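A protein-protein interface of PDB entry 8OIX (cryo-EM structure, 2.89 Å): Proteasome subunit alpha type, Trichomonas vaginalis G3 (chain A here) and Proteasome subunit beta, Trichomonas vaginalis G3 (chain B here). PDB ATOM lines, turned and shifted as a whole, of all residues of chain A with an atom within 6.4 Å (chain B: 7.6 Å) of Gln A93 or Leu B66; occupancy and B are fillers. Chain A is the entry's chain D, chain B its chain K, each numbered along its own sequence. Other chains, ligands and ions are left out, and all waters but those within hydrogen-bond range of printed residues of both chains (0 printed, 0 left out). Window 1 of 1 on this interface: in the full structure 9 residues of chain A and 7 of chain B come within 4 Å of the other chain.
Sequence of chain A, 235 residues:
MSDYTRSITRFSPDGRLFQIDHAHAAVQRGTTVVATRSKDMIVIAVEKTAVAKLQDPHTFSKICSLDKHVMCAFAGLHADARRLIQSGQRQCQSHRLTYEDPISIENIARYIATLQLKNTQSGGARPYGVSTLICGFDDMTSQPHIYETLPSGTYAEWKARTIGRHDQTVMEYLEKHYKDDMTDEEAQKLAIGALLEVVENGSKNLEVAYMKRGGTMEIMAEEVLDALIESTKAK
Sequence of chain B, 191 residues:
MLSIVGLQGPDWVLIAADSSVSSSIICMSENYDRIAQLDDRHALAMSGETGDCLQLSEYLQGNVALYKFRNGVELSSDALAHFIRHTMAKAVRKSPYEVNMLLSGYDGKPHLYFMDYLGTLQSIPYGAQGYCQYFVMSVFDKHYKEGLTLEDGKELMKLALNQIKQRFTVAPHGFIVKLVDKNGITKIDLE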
ATOM      1  N   LEU A  66      21.656  15.986  -9.517  1.00  0.00           N
ATOM      2  CA  LEU A  66      22.773  16.469  -8.715  1.00  0.00           C
ATOM      3  C   LEU A  66      23.233  15.423  -7.711  1.00  0.00           C
ATOM      4  O   LEU A  66      24.418  15.374  -7.365  1.00  0.00           O
ATOM      5  CB  LEU A  66      22.399  17.759  -7.991  1.00  0.00           C
ATOM      6  CG  LEU A  66      21.969  18.936  -8.860  1.00  0.00           C
ATOM      7  CD1 LEU A  66      21.744  20.156  -7.994  1.00  0.00           C
ATOM      8  CD2 LEU A  66      23.000  19.220  -9.935  1.00  0.00           C
ATOM      9  N   ASP A  67      22.318  14.582  -7.243  1.00  0.00           N
ATOM     10  CA  ASP A  67      22.639  13.535  -6.286  1.00  0.00           C
ATOM     11  C   ASP A  67      21.539  12.485  -6.367  1.00  0.00           C
ATOM     12  O   ASP A  67      20.565  12.638  -7.108  1.00  0.00           O
ATOM     13  CB  ASP A  67      22.786  14.107  -4.873  1.00  0.00           C
ATOM     14  CG  ASP A  67      23.635  13.232  -3.977  1.00  0.00           C
ATOM     15  OD1 ASP A  67      24.063  12.151  -4.431  1.00  0.00           O
ATOM     16  OD2 ASP A  67      23.878  13.627  -2.819  1.00  0.00           O
ATOM     17  N   LYS A  68      21.702  11.406  -5.599  1.00  0.00           N
ATOM     18  CA  LYS A  68      20.699  10.349  -5.597  1.00  0.00           C
ATOM     19  C   LYS A  68      19.371  10.818  -5.022  1.00  0.00           C
ATOM     20  O   LYS A  68      18.363  10.123  -5.185  1.00  0.00           O
ATOM     21  CB  LYS A  68      21.211   9.134  -4.823  1.00  0.00           C
ATOM     22  CG  LYS A  68      21.772   9.457  -3.457  1.00  0.00           C
ATOM     23  CD  LYS A  68      21.937   8.202  -2.618  1.00  0.00           C
ATOM     24  CE  LYS A  68      22.936   7.245  -3.248  1.00  0.00           C
ATOM     25  NZ  LYS A  68      24.303   7.831  -3.312  1.00  0.00           N
ATOM     26  N   GLN A  86      27.166  20.935 -12.837  1.00  0.00           N
ATOM     27  CA  GLN A  86      28.453  20.386 -12.431  1.00  0.00           C
ATOM     28  C   GLN A  86      28.840  20.859 -11.038  1.00  0.00           C
ATOM     29  O   GLN A  86      29.253  20.056 -10.191  1.00  0.00           O
ATOM     30  CB  GLN A  86      29.517  20.788 -13.451  1.00  0.00           C
ATOM     31  CG  GLN A  86      30.950  20.540 -13.027  1.00  0.00           C
ATOM     32  CD  GLN A  86      31.935  20.886 -14.125  1.00  0.00           C
ATOM     33  OE1 GLN A  86      33.035  21.369 -13.861  1.00  0.00           O
ATOM     34  NE2 GLN A  86      31.540  20.641 -15.369  1.00  0.00           N
ATOM     35  N   GLY A  88      26.761  21.925  -8.760  1.00  0.00           N
ATOM     36  CA  GLY A  88      25.810  21.355  -7.820  1.00  0.00           C
ATOM     37  C   GLY A  88      26.115  19.912  -7.472  1.00  0.00           C
ATOM     38  O   GLY A  88      25.972  19.500  -6.320  1.00  0.00           O
ATOM     39  N   GLN A  89      26.525  19.120  -8.463  1.00  0.00           N
ATOM     40  CA  GLN A  89      26.940  17.747  -8.194  1.00  0.00           C
ATOM     41  C   GLN A  89      28.192  17.717  -7.326  1.00  0.00           C
ATOM     42  O   GLN A  89      28.284  16.937  -6.367  1.00  0.00           O
ATOM     43  CB  GLN A  89      27.162  17.007  -9.512  1.00  0.00           C
ATOM     44  CG  GLN A  89      25.890  16.824 -10.317  1.00  0.00           C
ATOM     45  CD  GLN A  89      26.143  16.640 -11.795  1.00  0.00           C
ATOM     46  OE1 GLN A  89      27.225  16.938 -12.290  1.00  0.00           O
ATOM     47  NE2 GLN A  89      25.142  16.140 -12.508  1.00  0.00           N
ATOM     48  N   ARG A  90      29.174  18.565  -7.652  1.00  0.00           N
ATOM     49  CA  ARG A  90      30.352  18.687  -6.803  1.00  0.00           C
ATOM     50  C   ARG A  90      29.964  19.059  -5.379  1.00  0.00           C
ATOM     51  O   ARG A  90      30.538  18.540  -4.419  1.00  0.00           O
ATOM     52  CB  ARG A  90      31.319  19.721  -7.376  1.00  0.00           C
ATOM     53  CG  ARG A  90      31.983  19.312  -8.676  1.00  0.00           C
ATOM     54  CD  ARG A  90      32.703  20.492  -9.304  1.00  0.00           C
ATOM     55  NE  ARG A  90      33.621  20.080 -10.357  1.00  0.00           N
ATOM     56  CZ  ARG A  90      34.282  20.918 -11.142  1.00  0.00           C
ATOM     57  NH1 ARG A  90      34.129  22.228 -11.038  1.00  0.00           N
ATOM     58  NH2 ARG A  90      35.112  20.431 -12.060  1.00  0.00           N
ATOM     59  N   GLN A  91      28.987  19.951  -5.222  1.00  0.00           N
ATOM     60  CA  GLN A  91      28.589  20.392  -3.890  1.00  0.00           C
ATOM     61  C   GLN A  91      27.832  19.303  -3.146  1.00  0.00           C
ATOM     62  O   GLN A  91      27.968  19.178  -1.928  1.00  0.00           O
ATOM     63  CB  GLN A  91      27.739  21.655  -3.980  1.00  0.00           C
ATOM     64  CG  GLN A  91      27.112  22.092  -2.660  1.00  0.00           C
ATOM     65  CD  GLN A  91      28.123  22.576  -1.634  1.00  0.00           C
ATOM     66  OE1 GLN A  91      29.331  22.570  -1.872  1.00  0.00           O
ATOM     67  NE2 GLN A  91      27.627  23.002  -0.479  1.00  0.00           N
ATOM     68  N   CYS A  92      27.016  18.522  -3.849  1.00  0.00           N
ATOM     69  CA  CYS A  92      26.349  17.395  -3.208  1.00  0.00           C
ATOM     70  C   CYS A  92      27.374  16.400  -2.684  1.00  0.00           C
ATOM     71  O   CYS A  92      27.290  15.936  -1.537  1.00  0.00           O
ATOM     72  CB  CYS A  92      25.391  16.720  -4.190  1.00  0.00           C
ATOM     73  SG  CYS A  92      23.970  17.725  -4.670  1.00  0.00           S
ATOM     74  N   GLN A  93      28.379  16.088  -3.503  1.00  0.00           N
ATOM     75  CA  GLN A  93      29.407  15.154  -3.056  1.00  0.00           C
ATOM     76  C   GLN A  93      30.276  15.753  -1.957  1.00  0.00           C
ATOM     77  O   GLN A  93      30.708  15.034  -1.052  1.00  0.00           O
ATOM     78  CB  GLN A  93      30.254  14.705  -4.242  1.00  0.00           C
ATOM     79  CG  GLN A  93      29.434  14.059  -5.342  1.00  0.00           C
ATOM     80  CD  GLN A  93      28.468  13.011  -4.817  1.00  0.00           C
ATOM     81  OE1 GLN A  93      28.789  12.251  -3.902  1.00  0.00           O
ATOM     82  NE2 GLN A  93      27.272  12.971  -5.391  1.00  0.00           N
ATOM     83  N   SER A  94      30.515  17.065  -1.994  1.00  0.00           N
ATOM     84  CA  SER A  94      31.293  17.706  -0.941  1.00  0.00           C
ATOM     85  C   SER A  94      30.511  17.777   0.362  1.00  0.00           C
ATOM     86  O   SER A  94      31.097  17.665   1.442  1.00  0.00           O
ATOM     87  CB  SER A  94      31.724  19.103  -1.386  1.00  0.00           C
ATOM     88  OG  SER A  94      32.802  19.579  -0.601  1.00  0.00           O
ATOM     89  N   HIS A  95      29.195  17.967   0.281  1.00  0.00           N
ATOM     90  CA  HIS A  95      28.353  17.910   1.467  1.00  0.00           C
ATOM     91  C   HIS A  95      28.341  16.509   2.055  1.00  0.00           C
ATOM     92  O   HIS A  95      28.328  16.344   3.278  1.00  0.00           O
ATOM     93  CB  HIS A  95      26.936  18.367   1.121  1.00  0.00           C
ATOM     94  CG  HIS A  95      26.058  18.577   2.314  1.00  0.00           C
ATOM     95  ND1 HIS A  95      25.506  17.535   3.027  1.00  0.00           N
ATOM     96  CD2 HIS A  95      25.632  19.711   2.918  1.00  0.00           C
ATOM     97  CE1 HIS A  95      24.782  18.018   4.020  1.00  0.00           C
ATOM     98  NE2 HIS A  95      24.843  19.336   3.976  1.00  0.00           N
ATOM     99  N   ARG A  96      28.331  15.484   1.200  1.00  0.00           N
ATOM    100  CA  ARG A  96      28.487  14.121   1.698  1.00  0.00           C
ATOM    101  C   ARG A  96      29.848  13.926   2.360  1.00  0.00           C
ATOM    102  O   ARG A  96      29.955  13.260   3.395  1.00  0.00           O
ATOM    103  CB  ARG A  96      28.283  13.120   0.563  1.00  0.00           C
ATOM    104  CG  ARG A  96      26.855  13.072   0.067  1.00  0.00           C
ATOM    105  CD  ARG A  96      26.645  11.971  -0.947  1.00  0.00           C
ATOM    106  NE  ARG A  96      25.251  11.905  -1.363  1.00  0.00           N
ATOM    107  CZ  ARG A  96      24.300  11.277  -0.686  1.00  0.00           C
ATOM    108  NH1 ARG A  96      24.559  10.651   0.449  1.00  0.00           N
ATOM    109  NH2 ARG A  96      23.057  11.287  -1.154  1.00  0.00           N
ATOM    110  N   LEU A  97      30.902  14.487   1.766  1.00  0.00           N
ATOM    111  CA  LEU A  97      32.236  14.370   2.347  1.00  0.00           C
ATOM    112  C   LEU A  97      32.310  15.046   3.709  1.00  0.00           C
ATOM    113  O   LEU A  97      32.929  14.522   4.643  1.00  0.00           O
ATOM    114  CB  LEU A  97      33.269  14.986   1.406  1.00  0.00           C
ATOM    115  CG  LEU A  97      33.606  14.238   0.122  1.00  0.00           C
ATOM    116  CD1 LEU A  97      34.312  15.155  -0.859  1.00  0.00           C
ATOM    117  CD2 LEU A  97      34.488  13.072   0.468  1.00  0.00           C
ATOM    118  N   THR A  98      31.692  16.217   3.835  1.00  0.00           N
ATOM    119  CA  THR A  98      31.798  17.030   5.037  1.00  0.00           C
ATOM    120  C   THR A  98      30.814  16.620   6.125  1.00  0.00           C
ATOM    121  O   THR A  98      31.073  16.879   7.305  1.00  0.00           O
ATOM    122  CB  THR A  98      31.588  18.500   4.668  1.00  0.00           C
ATOM    123  OG1 THR A  98      32.298  18.790   3.458  1.00  0.00           O
ATOM    124  CG2 THR A  98      32.130  19.398   5.750  1.00  0.00           C
ATOM    125  N   ILE A 103      22.781  16.057   1.064  1.00  0.00           N
ATOM    126  CA  ILE A 103      22.613  17.501   1.143  1.00  0.00           C
ATOM    127  C   ILE A 103      21.131  17.841   1.136  1.00  0.00           C
ATOM    128  O   ILE A 103      20.350  17.290   0.351  1.00  0.00           O
ATOM    129  CB  ILE A 103      23.370  18.193  -0.001  1.00  0.00           C
ATOM    130  CG1 ILE A 103      23.323  19.713   0.167  1.00  0.00           C
ATOM    131  CG2 ILE A 103      22.820  17.777  -1.353  1.00  0.00           C
ATOM    132  CD1 ILE A 103      24.288  20.453  -0.726  1.00  0.00           C
ATOM    133  N   GLU B  58      35.654   7.948   1.746  1.00  0.00           N
ATOM    134  CA  GLU B  58      34.688   9.001   1.470  1.00  0.00           C
ATOM    135  C   GLU B  58      35.075   9.783   0.226  1.00  0.00           C
ATOM    136  O   GLU B  58      34.214  10.103  -0.599  1.00  0.00           O
ATOM    137  CB  GLU B  58      34.571   9.921   2.679  1.00  0.00           C
ATOM    138  CG  GLU B  58      34.045   9.220   3.914  1.00  0.00           C
ATOM    139  CD  GLU B  58      34.554   9.850   5.189  1.00  0.00           C
ATOM    140  OE1 GLU B  58      35.133  10.954   5.112  1.00  0.00           O
ATOM    141  OE2 GLU B  58      34.378   9.244   6.267  1.00  0.00           O
ATOM    142  N   TYR B  59      36.365  10.085   0.063  1.00  0.00           N
ATOM    143  CA  TYR B  59      36.817  10.779  -1.137  1.00  0.00           C
ATOM    144  C   TYR B  59      36.521   9.961  -2.388  1.00  0.00           C
ATOM    145  O   TYR B  59      35.987  10.484  -3.373  1.00  0.00           O
ATOM    146  CB  TYR B  59      38.310  11.090  -1.023  1.00  0.00           C
ATOM    147  CG  TYR B  59      38.944  11.645  -2.280  1.00  0.00           C
ATOM    148  CD1 TYR B  59      39.508  10.803  -3.231  1.00  0.00           C
ATOM    149  CD2 TYR B  59      38.978  13.012  -2.515  1.00  0.00           C
ATOM    150  CE1 TYR B  59      40.087  11.307  -4.377  1.00  0.00           C
ATOM    151  CE2 TYR B  59      39.556  13.524  -3.659  1.00  0.00           C
ATOM    152  CZ  TYR B  59      40.107  12.668  -4.586  1.00  0.00           C
ATOM    153  OH  TYR B  59      40.683  13.177  -5.727  1.00  0.00           O
ATOM    154  N   LEU B  60      36.853   8.669  -2.362  1.00  0.00           N
ATOM    155  CA  LEU B  60      36.633   7.828  -3.534  1.00  0.00           C
ATOM    156  C   LEU B  60      35.149   7.652  -3.827  1.00  0.00           C
ATOM    157  O   LEU B  60      34.739   7.687  -4.990  1.00  0.00           O
ATOM    158  CB  LEU B  60      37.314   6.475  -3.349  1.00  0.00           C
ATOM    159  CG  LEU B  60      38.840   6.539  -3.292  1.00  0.00           C
ATOM    160  CD1 LEU B  60      39.407   5.241  -2.759  1.00  0.00           C
ATOM    161  CD2 LEU B  60      39.410   6.853  -4.664  1.00  0.00           C
ATOM    162  N   GLN B  61      34.328   7.455  -2.794  1.00  0.00           N
ATOM    163  CA  GLN B  61      32.892   7.312  -3.006  1.00  0.00           C
ATOM    164  C   GLN B  61      32.285   8.598  -3.551  1.00  0.00           C
ATOM    165  O   GLN B  61      31.444   8.558  -4.457  1.00  0.00           O
ATOM    166  CB  GLN B  61      32.211   6.903  -1.701  1.00  0.00           C
ATOM    167  CG  GLN B  61      30.696   6.907  -1.763  1.00  0.00           C
ATOM    168  CD  GLN B  61      30.066   6.236  -0.562  1.00  0.00           C
ATOM    169  OE1 GLN B  61      28.884   5.892  -0.579  1.00  0.00           O
ATOM    170  NE2 GLN B  61      30.855   6.044   0.488  1.00  0.00           N
ATOM    171  N   GLY B  62      32.699   9.745  -3.011  1.00  0.00           N
ATOM    172  CA  GLY B  62      32.229  11.011  -3.538  1.00  0.00           C
ATOM    173  C   GLY B  62      32.631  11.215  -4.982  1.00  0.00           C
ATOM    174  O   GLY B  62      31.843  11.700  -5.791  1.00  0.00           O
ATOM    175  N   ASN B  63      33.863  10.837  -5.331  1.00  0.00           N
ATOM    176  CA  ASN B  63      34.313  10.980  -6.710  1.00  0.00           C
ATOM    177  C   ASN B  63      33.576  10.026  -7.644  1.00  0.00           C
ATOM    178  O   ASN B  63      33.273  10.383  -8.785  1.00  0.00           O
ATOM    179  CB  ASN B  63      35.820  10.761  -6.792  1.00  0.00           C
ATOM    180  CG  ASN B  63      36.606  11.991  -6.400  1.00  0.00           C
ATOM    181  OD1 ASN B  63      36.807  12.895  -7.209  1.00  0.00           O
ATOM    182  ND2 ASN B  63      37.050  12.034  -5.152  1.00  0.00           N
ATOM    183  N   VAL B  64      33.279   8.810  -7.183  1.00  0.00           N
ATOM    184  CA  VAL B  64      32.519   7.871  -8.003  1.00  0.00           C
ATOM    185  C   VAL B  64      31.112   8.398  -8.246  1.00  0.00           C
ATOM    186  O   VAL B  64      30.604   8.370  -9.375  1.00  0.00           O
ATOM    187  CB  VAL B  64      32.490   6.479  -7.349  1.00  0.00           C
ATOM    188  CG1 VAL B  64      31.535   5.566  -8.095  1.00  0.00           C
ATOM    189  CG2 VAL B  64      33.872   5.879  -7.338  1.00  0.00           C
ATOM    190  N   ALA B  65      30.461   8.893  -7.192  1.00  0.00           N
ATOM    191  CA  ALA B  65      29.130   9.464  -7.355  1.00  0.00           C
ATOM    192  C   ALA B  65      29.174  10.696  -8.249  1.00  0.00           C
ATOM    193  O   ALA B  65      28.275  10.912  -9.068  1.00  0.00           O
ATOM    194  CB  ALA B  65      28.529   9.799  -5.993  1.00  0.00           C
ATOM    195  N   LEU B  66      30.219  11.513  -8.111  1.00  0.00           N
ATOM    196  CA  LEU B  66      30.351  12.702  -8.938  1.00  0.00           C
ATOM    197  C   LEU B  66      30.571  12.334 -10.397  1.00  0.00           C
ATOM    198  O   LEU B  66      30.098  13.042 -11.287  1.00  0.00           O
ATOM    199  CB  LEU B  66      31.497  13.570  -8.422  1.00  0.00           C
ATOM    200  CG  LEU B  66      31.784  14.878  -9.157  1.00  0.00           C
ATOM    201  CD1 LEU B  66      30.564  15.774  -9.135  1.00  0.00           C
ATOM    202  CD2 LEU B  66      32.979  15.580  -8.537  1.00  0.00           C
ATOM    203  N   TYR B  67      31.294  11.247 -10.663  1.00  0.00           N
ATOM    204  CA  TYR B  67      31.441  10.776 -12.036  1.00  0.00           C
ATOM    205  C   TYR B  67      30.111  10.258 -12.569  1.00  0.00           C
ATOM    206  O   TYR B  67      29.776  10.469 -13.739  1.00  0.00           O
ATOM    207  CB  TYR B  67      32.516   9.691 -12.106  1.00  0.00           C
ATOM    208  CG  TYR B  67      32.732   9.108 -13.484  1.00  0.00           C
ATOM    209  CD1 TYR B  67      31.959   8.051 -13.947  1.00  0.00           C
ATOM    210  CD2 TYR B  67      33.722   9.607 -14.319  1.00  0.00           C
ATOM    211  CE1 TYR B  67      32.158   7.518 -15.203  1.00  0.00           C
ATOM    212  CE2 TYR B  67      33.929   9.078 -15.575  1.00  0.00           C
ATOM    213  CZ  TYR B  67      33.145   8.035 -16.012  1.00  0.00           C
ATOM    214  OH  TYR B  67      33.348   7.504 -17.264  1.00  0.00           O
ATOM    215  N   LYS B  68      29.345   9.571 -11.718  1.00  0.00           N
ATOM    216  CA  LYS B  68      28.050   9.036 -12.126  1.00  0.00           C
ATOM    217  C   LYS B  68      27.048  10.147 -12.408  1.00  0.00           C
ATOM    218  O   LYS B  68      26.133   9.967 -13.221  1.00  0.00           O
ATOM    219  CB  LYS B  68      27.506   8.104 -11.043  1.00  0.00           C
ATOM    220  CG  LYS B  68      26.151   7.497 -11.361  1.00  0.00           C
ATOM    221  CD  LYS B  68      25.653   6.641 -10.214  1.00  0.00           C
ATOM    222  CE  LYS B  68      25.373   7.486  -8.986  1.00  0.00           C
ATOM    223  NZ  LYS B  68      24.837   6.672  -7.863  1.00  0.00           N
ATOM    224  N   PHE B  69      27.176  11.277 -11.723  1.00  0.00           N
ATOM    225  CA  PHE B  69      26.227  12.373 -11.872  1.00  0.00           C
ATOM    226  C   PHE B  69      26.654  13.362 -12.951  1.00  0.00           C
ATOM    227  O   PHE B  69      25.813  13.838 -13.719  1.00  0.00           O
ATOM    228  CB  PHE B  69      26.038  13.063 -10.522  1.00  0.00           C
ATOM    229  CG  PHE B  69      25.311  12.212  -9.527  1.00  0.00           C
ATOM    230  CD1 PHE B  69      24.253  11.418  -9.929  1.00  0.00           C
ATOM    231  CD2 PHE B  69      25.712  12.162  -8.205  1.00  0.00           C
ATOM    232  CE1 PHE B  69      23.589  10.615  -9.028  1.00  0.00           C
ATOM    233  CE2 PHE B  69      25.057  11.353  -7.301  1.00  0.00           C
ATOM    234  CZ  PHE B  69      23.991  10.582  -7.713  1.00  0.00           C
ATOM    235  N   ARG B  70      27.948  13.683 -13.015  1.00  0.00           N
ATOM    236  CA  ARG B  70      28.464  14.549 -14.069  1.00  0.00           C
ATOM    237  C   ARG B  70      28.216  13.933 -15.437  1.00  0.00           C
ATOM    238  O   ARG B  70      27.710  14.592 -16.353  1.00  0.00           O
ATOM    239  CB  ARG B  70      29.963  14.771 -13.864  1.00  0.00           C
ATOM    240  CG  ARG B  70      30.328  15.787 -12.811  1.00  0.00           C
ATOM    241  CD  ARG B  70      30.161  17.181 -13.357  1.00  0.00           C
ATOM    242  NE  ARG B  70      31.128  17.465 -14.411  1.00  0.00           N
ATOM    243  CZ  ARG B  70      32.439  17.552 -14.229  1.00  0.00           C
ATOM    244  NH1 ARG B  70      32.967  17.617 -13.017  1.00  0.00           N
ATOM    245  NH2 ARG B  70      33.234  17.652 -15.290  1.00  0.00           N
ATOM    246  N   ASN B  71      28.564  12.663 -15.583  1.00  0.00           N
ATOM    247  CA  ASN B  71      28.354  11.903 -16.799  1.00  0.00           C
ATOM    248  C   ASN B  71      27.346  10.809 -16.490  1.00  0.00           C
ATOM    249  O   ASN B  71      27.444  10.149 -15.454  1.00  0.00           O
ATOM    250  CB  ASN B  71      29.669  11.296 -17.281  1.00  0.00           C
ATOM    251  CG  ASN B  71      30.862  12.168 -16.943  1.00  0.00           C
ATOM    252  OD1 ASN B  71      30.970  13.301 -17.411  1.00  0.00           O
ATOM    253  ND2 ASN B  71      31.758  11.648 -16.115  1.00  0.00           N
ATOM    254  N   GLY B  72      26.402  10.583 -17.394  1.00  0.00           N
ATOM    255  CA  GLY B  72      25.337   9.656 -17.063  1.00  0.00           C
ATOM    256  C   GLY B  72      25.766   8.214 -17.221  1.00  0.00           C
ATOM    257  O   GLY B  72      25.027   7.385 -17.762  1.00  0.00           O
ATOM    258  N   VAL B  73      26.966   7.909 -16.732  1.00  0.00           N
ATOM    259  CA  VAL B  73      27.569   6.587 -16.837  1.00  0.00           C
ATOM    260  C   VAL B  73      28.330   6.305 -15.549  1.00  0.00           C
ATOM    261  O   VAL B  73      28.950   7.203 -14.970  1.00  0.00           O
ATOM    262  CB  VAL B  73      28.499   6.481 -18.063  1.00  0.00           C
ATOM    263  CG1 VAL B  73      27.707   6.661 -19.342  1.00  0.00           C
ATOM    264  CG2 VAL B  73      29.615   7.511 -17.987  1.00  0.00           C
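The backbone carbonyl oxygen (O) of Tyr B59 lies within hydrogen-bond range of the side-chain amide nitrogen (ND2) of Asn B63 (2.6 Å). O of Leu A66 sits close to SG of Cys A92. The side-chain amide nitrogen (NE2) of Gln A93 lies within hydrogen-bond range of the side-chain carboxylate (OD1) of Asp A67. The side-chain carboxylate (OD2) of Asp A67 is in salt-bridge range of the guanidinium group (NE) of Arg A96, 2.6 Å away. The guanidinium group (NH2) of Arg A90 sits at hydrogen-bond distance from the side-chain amide oxygen (OE1) of Gln A86 (2.9 Å).
Of the printed residues of chain B, Gln A86 touches Arg B70. Gln A93 touches four residues of chain B. Of the printed residues of chain A, Tyr B59 touches Leu A97. Leu B60 touches none of the printed residues of chain A. Of chain A, only Gln A89 (3.6 Å), Arg A90 (3.5 Å) and Gln A93 (3.7 Å) come within 4 Å of Leu B66. Of the printed residues of chain A, Arg B70 touches Gln A86, Gln A89 and Arg A90. The nearest printed residue of chain B that does not touch Gln A86 is Leu B66 (4.6 Å).
Hydrophobic or aromatic side chains of chain B that line the printed part of chain A: Ala B65, Leu B66 and Phe B69. Along chain B the printed residues that touch a printed residue of chain A span positions 58 to 70.
O of Phe B69 lies within hydrogen-bond range of NE2 of Gln A89 (2.7 Å). The guanidinium group (NE) of Arg B70 sits close to the side-chain amide nitrogen (NE2) of Gln A86 (3.3 Å). The backbone NH (N) of Arg B70 lies close to the side-chain amide oxygen (OE1) of Gln A89, at 3.4 Å.
Phe B69 touches Leu A66 (CD2 to O, 3.6 Å). OD1 of Asp A67 touches CE2 of Phe B69, at 3.1 Å. Lys A68 touches Phe B69. N of Arg A90 touches CD1 of Leu B66, at 3.5 Å. Arg B70 touches Arg A90 (NH1 to NH2, 3.7 Å). Gln A93 touches Gly B62 (CG to O, 3.4 Å). CB of Ala B65 touches OE1 of Gln A93, at 3.2 Å. NE2 of Gln A93 touches CD2 of Phe B69, at 3.3 Å. Leu A97 touches Glu B58 (CD2 to O, 3.2 Å). N of Tyr B59 touches CD2 of Leu A97 (3.6 Å).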
